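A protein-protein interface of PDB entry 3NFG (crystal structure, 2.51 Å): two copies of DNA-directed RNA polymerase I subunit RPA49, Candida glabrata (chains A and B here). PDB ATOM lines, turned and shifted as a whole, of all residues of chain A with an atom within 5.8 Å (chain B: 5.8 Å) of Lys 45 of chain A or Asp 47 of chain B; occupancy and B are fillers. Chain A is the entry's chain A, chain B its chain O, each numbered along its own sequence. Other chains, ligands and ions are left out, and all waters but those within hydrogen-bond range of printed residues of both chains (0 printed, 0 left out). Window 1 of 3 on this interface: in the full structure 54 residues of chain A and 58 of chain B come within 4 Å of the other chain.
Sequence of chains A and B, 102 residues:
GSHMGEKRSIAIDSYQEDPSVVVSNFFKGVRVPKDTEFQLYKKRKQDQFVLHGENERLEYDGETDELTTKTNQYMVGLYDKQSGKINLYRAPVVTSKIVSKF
N of Lys 43 of chain A lies within hydrogen-bond range of O of Gln 48 of chain B, at 2.8 Å.
The side-chain amino group (NZ) of Lys 45 of chain A lies within salt-bridge range of the side-chain carboxylate (OD2) of Asp 47 of chain A, 2.8 Å away.
The side-chain hydroxyl (OG1) of Thr 69 of chain B is in hydrogen-bond range of the backbone carbonyl oxygen (O) of Asp 47 of chain B.
N of Phe 49 of chain B is in hydrogen-bond range of OG1 of Thr 64 of chain B (3.0 Å).
Among the printed residues, pairs that only touch across the chains: Lys 45 of chain A with Asp 47 of chain B (3.3 Å), Lys 42 of chain A with Gln 48 of chain B (3.4 Å), Lys 42 of chain A with Asp 47 of chain B (3.5 Å), Lys 45 of chain A with Lys 45 of chain B (3.6 Å), Asp 47 of chain A with Lys 42 of chain B (3.6 Å), Lys 43 of chain A with Asp 47 of chain B (3.8 Å) and Lys 42 of chain A with Phe 49 of chain B (3.98 Å).
Printed residues of chain B within 4 Å of Lys 42 of chain A: Asp 47 (3.5 Å), Gln 48 (3.4 Å) and Phe 49 (3.98 Å).
Of the printed residues of chain B, Lys 43 of chain A touches Asp 47 and Gln 48.
Asp 47 of chain B touches just these residues of chain A: Lys 42 (3.5 Å), Lys 43 (3.8 Å) and Lys 45 (3.3 Å).
Of the printed residues of chain A, Gln 48 of chain B touches Lys 42 (3.4 Å) and Lys 43 (2.8 Å).
The nearest residue of chain B that does not touch Lys 45 of chain A is Lys 42 of chain B (4.7 Å).
Of the 8 printed residues of chain B, 5 touch a printed residue of chain A.
Printed residues of chain B that touch a printed residue of chain A: Lys 42, Lys 45, Asp 47, Gln 48 and Phe 49.
Among the printed residues, no Asp or Glu carboxylate lies within 4 Å of a Lys or Arg side-chain nitrogen of the other chain.
Lys 42 of chain A touches Asp 47 of chain B, and with the chains exchanged Asp 47 of chain A touches Lys 42 of chain B.
Lys 45 of chain B touches its own counterpart, Lys 45 of chain A.
Lys 45 of chain A touches Asp 47 of chain B, but with the chains exchanged Asp 47 of chain A does not touch Lys 45 of chain B (4.4 Å).
Of the 8 pairs that touch across the chains among the printed residues, 3 have their exchanged pair printed and touching as well.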
ATOM      1  N   LYS A  42      -4.126  28.909  16.975  1.00  0.00           N
ATOM      2  CA  LYS A  42      -3.499  28.243  15.827  1.00  0.00           C
ATOM      3  C   LYS A  42      -1.998  28.510  15.825  1.00  0.00           C
ATOM      4  O   LYS A  42      -1.578  29.625  16.141  1.00  0.00           O
ATOM      5  CB  LYS A  42      -4.164  28.820  14.562  1.00  0.00           C
ATOM      6  CG  LYS A  42      -3.731  28.287  13.213  1.00  0.00           C
ATOM      7  CD  LYS A  42      -4.367  29.132  12.043  1.00  0.00           C
ATOM      8  CE  LYS A  42      -3.975  30.623  11.998  1.00  0.00           C
ATOM      9  NZ  LYS A  42      -3.975  31.213  10.628  1.00  0.00           N
ATOM     10  N   LYS A  43      -1.185  27.497  15.462  1.00  0.00           N
ATOM     11  CA  LYS A  43       0.264  27.695  15.386  1.00  0.00           C
ATOM     12  C   LYS A  43       0.581  28.536  14.143  1.00  0.00           C
ATOM     13  O   LYS A  43       0.016  28.289  13.063  1.00  0.00           O
ATOM     14  CB  LYS A  43       1.045  26.371  15.347  1.00  0.00           C
ATOM     15  CG  LYS A  43       2.570  26.545  15.570  1.00  0.00           C
ATOM     16  CD  LYS A  43       3.300  25.227  15.463  1.00  0.00           C
ATOM     17  CE  LYS A  43       4.758  25.314  15.818  1.00  0.00           C
ATOM     18  NZ  LYS A  43       5.454  24.040  15.502  1.00  0.00           N
ATOM     19  N   ARG A  44       1.443  29.559  14.334  1.00  0.00           N
ATOM     20  CA  ARG A  44       1.849  30.457  13.271  1.00  0.00           C
ATOM     21  C   ARG A  44       2.714  29.689  12.305  1.00  0.00           C
ATOM     22  O   ARG A  44       3.744  29.152  12.695  1.00  0.00           O
ATOM     23  CB  ARG A  44       2.549  31.733  13.796  1.00  0.00           C
ATOM     24  CG  ARG A  44       1.619  32.738  14.501  1.00  0.00           C
ATOM     25  CD  ARG A  44       2.259  34.076  14.791  1.00  0.00           C
ATOM     26  NE  ARG A  44       2.086  34.960  13.648  1.00  0.00           N
ATOM     27  CZ  ARG A  44       3.086  35.542  13.001  1.00  0.00           C
ATOM     28  NH1 ARG A  44       4.334  35.393  13.426  1.00  0.00           N
ATOM     29  NH2 ARG A  44       2.845  36.334  11.966  1.00  0.00           N
ATOM     30  N   LYS A  45       2.213  29.528  11.078  1.00  0.00           N
ATOM     31  CA  LYS A  45       2.926  28.884   9.994  1.00  0.00           C
ATOM     32  C   LYS A  45       3.201  29.906   8.862  1.00  0.00           C
ATOM     33  O   LYS A  45       2.737  31.049   8.882  1.00  0.00           O
ATOM     34  CB  LYS A  45       2.196  27.628   9.476  1.00  0.00           C
ATOM     35  CG  LYS A  45       0.818  27.901   8.866  1.00  0.00           C
ATOM     36  CD  LYS A  45       0.356  26.777   7.931  1.00  0.00           C
ATOM     37  CE  LYS A  45      -1.078  26.913   7.458  1.00  0.00           C
ATOM     38  NZ  LYS A  45      -1.252  27.973   6.432  1.00  0.00           N
ATOM     39  N   GLN A  46       4.011  29.490   7.919  1.00  0.00           N
ATOM     40  CA  GLN A  46       4.336  30.205   6.708  1.00  0.00           C
ATOM     41  C   GLN A  46       4.141  29.138   5.679  1.00  0.00           C
ATOM     42  O   GLN A  46       4.603  27.995   5.893  1.00  0.00           O
ATOM     43  CB  GLN A  46       5.799  30.632   6.712  1.00  0.00           C
ATOM     44  CG  GLN A  46       6.037  32.007   7.309  1.00  0.00           C
ATOM     45  CD  GLN A  46       5.721  33.083   6.329  1.00  0.00           C
ATOM     46  OE1 GLN A  46       6.001  32.978   5.128  1.00  0.00           O
ATOM     47  NE2 GLN A  46       5.112  34.130   6.831  1.00  0.00           N
ATOM     48  N   ASP A  47       3.394  29.456   4.615  1.00  0.00           N
ATOM     49  CA  ASP A  47       3.146  28.463   3.587  1.00  0.00           C
ATOM     50  C   ASP A  47       4.291  28.346   2.591  1.00  0.00           C
ATOM     51  O   ASP A  47       5.121  29.231   2.510  1.00  0.00           O
ATOM     52  CB  ASP A  47       1.800  28.708   2.890  1.00  0.00           C
ATOM     53  CG  ASP A  47       0.586  28.238   3.678  1.00  0.00           C
ATOM     54  OD1 ASP A  47       0.391  26.996   3.798  1.00  0.00           O
ATOM     55  OD2 ASP A  47      -0.213  29.105   4.116  1.00  0.00           O
ATOM     56  N   ARG A  90       0.518  40.075   2.699  1.00  0.00           N
ATOM     57  CA  ARG A  90       1.494  39.016   2.894  1.00  0.00           C
ATOM     58  C   ARG A  90       1.774  38.350   1.529  1.00  0.00           C
ATOM     59  O   ARG A  90       0.843  38.101   0.738  1.00  0.00           O
ATOM     60  CB  ARG A  90       0.976  38.003   3.911  1.00  0.00           C
ATOM     61  CG  ARG A  90       2.022  36.999   4.313  1.00  0.00           C
ATOM     62  CD  ARG A  90       1.436  36.004   5.251  1.00  0.00           C
ATOM     63  NE  ARG A  90       2.229  35.976   6.471  1.00  0.00           N
ATOM     64  CZ  ARG A  90       2.065  35.091   7.444  1.00  0.00           C
ATOM     65  NH1 ARG A  90       1.124  34.158   7.349  1.00  0.00           N
ATOM     66  NH2 ARG A  90       2.841  35.126   8.520  1.00  0.00           N
ATOM     67  N   LYS B  42      -0.269  26.037  -3.541  1.00  0.00           N
ATOM     68  CA  LYS B  42       0.101  26.003  -2.131  1.00  0.00           C
ATOM     69  C   LYS B  42       0.298  24.555  -1.657  1.00  0.00           C
ATOM     70  O   LYS B  42      -0.520  23.695  -1.974  1.00  0.00           O
ATOM     71  CB  LYS B  42      -1.001  26.700  -1.309  1.00  0.00           C
ATOM     72  CG  LYS B  42      -0.677  26.892   0.173  1.00  0.00           C
ATOM     73  CD  LYS B  42      -1.806  27.574   0.946  1.00  0.00           C
ATOM     74  CE  LYS B  42      -2.984  26.686   1.238  1.00  0.00           C
ATOM     75  NZ  LYS B  42      -3.680  27.123   2.481  1.00  0.00           N
ATOM     76  N   LYS B  45      -0.335  21.959   3.998  1.00  0.00           N
ATOM     77  CA  LYS B  45       0.255  22.011   5.329  1.00  0.00           C
ATOM     78  C   LYS B  45      -0.863  22.312   6.303  1.00  0.00           C
ATOM     79  O   LYS B  45      -1.318  23.468   6.384  1.00  0.00           O
ATOM     80  CB  LYS B  45       1.371  23.067   5.461  1.00  0.00           C
ATOM     81  CG  LYS B  45       1.909  23.168   6.903  1.00  0.00           C
ATOM     82  CD  LYS B  45       3.009  24.191   7.078  1.00  0.00           C
ATOM     83  CE  LYS B  45       3.594  24.109   8.464  1.00  0.00           C
ATOM     84  NZ  LYS B  45       4.769  25.004   8.602  1.00  0.00           N
ATOM     85  N   GLN B  46      -1.279  21.265   7.053  1.00  0.00           N
ATOM     86  CA  GLN B  46      -2.336  21.270   8.062  1.00  0.00           C
ATOM     87  C   GLN B  46      -1.923  21.926   9.405  1.00  0.00           C
ATOM     88  O   GLN B  46      -0.833  21.657   9.923  1.00  0.00           O
ATOM     89  CB  GLN B  46      -2.862  19.848   8.267  1.00  0.00           C
ATOM     90  CG  GLN B  46      -4.272  19.800   8.836  1.00  0.00           C
ATOM     91  CD  GLN B  46      -4.785  18.391   8.870  1.00  0.00           C
ATOM     92  OE1 GLN B  46      -4.621  17.619   7.912  1.00  0.00           O
ATOM     93  NE2 GLN B  46      -5.433  18.035   9.973  1.00  0.00           N
ATOM     94  N   ASP B  47      -2.828  22.757   9.966  1.00  0.00           N
ATOM     95  CA  ASP B  47      -2.621  23.531  11.184  1.00  0.00           C
ATOM     96  C   ASP B  47      -2.605  22.750  12.500  1.00  0.00           C
ATOM     97  O   ASP B  47      -3.186  21.683  12.618  1.00  0.00           O
ATOM     98  CB  ASP B  47      -3.597  24.715  11.260  1.00  0.00           C
ATOM     99  CG  ASP B  47      -3.283  25.857  10.322  1.00  0.00           C
ATOM    100  OD1 ASP B  47      -2.267  26.559  10.560  1.00  0.00           O
ATOM    101  OD2 ASP B  47      -4.111  26.125   9.423  1.00  0.00           O
ATOM    102  N   GLN B  48      -1.902  23.308  13.477  1.00  0.00           N
ATOM    103  CA  GLN B  48      -1.787  22.802  14.829  1.00  0.00           C
ATOM    104  C   GLN B  48      -2.522  23.791  15.746  1.00  0.00           C
ATOM    105  O   GLN B  48      -2.425  25.014  15.552  1.00  0.00           O
ATOM    106  CB  GLN B  48      -0.317  22.691  15.227  1.00  0.00           C
ATOM    107  CG  GLN B  48       0.416  21.533  14.579  1.00  0.00           C
ATOM    108  CD  GLN B  48       1.741  21.320  15.240  1.00  0.00           C
ATOM    109  OE1 GLN B  48       2.737  21.924  14.881  1.00  0.00           O
ATOM    110  NE2 GLN B  48       1.763  20.507  16.271  1.00  0.00           N
ATOM    111  N   PHE B  49      -3.266  23.280  16.716  1.00  0.00           N
ATOM    112  CA  PHE B  49      -4.056  24.143  17.599  1.00  0.00           C
ATOM    113  C   PHE B  49      -3.865  23.908  19.067  1.00  0.00           C
ATOM    114  O   PHE B  49      -3.562  22.793  19.486  1.00  0.00           O
ATOM    115  CB  PHE B  49      -5.564  23.974  17.302  1.00  0.00           C
ATOM    116  CG  PHE B  49      -6.010  24.381  15.909  1.00  0.00           C
ATOM    117  CD1 PHE B  49      -6.569  25.635  15.676  1.00  0.00           C
ATOM    118  CD2 PHE B  49      -5.881  23.512  14.835  1.00  0.00           C
ATOM    119  CE1 PHE B  49      -6.975  26.008  14.384  1.00  0.00           C
ATOM    120  CE2 PHE B  49      -6.293  23.886  13.554  1.00  0.00           C
ATOM    121  CZ  PHE B  49      -6.845  25.123  13.337  1.00  0.00           C
ATOM    122  N   THR B  64      -3.573  19.725  19.700  1.00  0.00           N
ATOM    123  CA  THR B  64      -3.629  18.730  18.613  1.00  0.00           C
ATOM    124  C   THR B  64      -2.312  17.900  18.736  1.00  0.00           C
ATOM    125  O   THR B  64      -1.339  18.374  19.351  1.00  0.00           O
ATOM    126  CB  THR B  64      -3.678  19.422  17.218  1.00  0.00           C
ATOM    127  OG1 THR B  64      -2.632  20.371  17.105  1.00  0.00           O
ATOM    128  CG2 THR B  64      -4.980  20.127  16.938  1.00  0.00           C
ATOM    129  N   THR B  69      -1.601  15.496  12.919  1.00  0.00           N
ATOM    130  CA  THR B  69      -1.745  16.691  12.091  1.00  0.00           C
ATOM    131  C   THR B  69      -1.080  16.490  10.655  1.00  0.00           C
ATOM    132  O   THR B  69      -1.506  17.117   9.665  1.00  0.00           O
ATOM    133  CB  THR B  69      -1.202  17.879  12.933  1.00  0.00           C
ATOM    134  OG1 THR B  69      -2.292  18.668  13.424  1.00  0.00           O
ATOM    135  CG2 THR B  69      -0.125  18.737  12.215  1.00  0.00           C
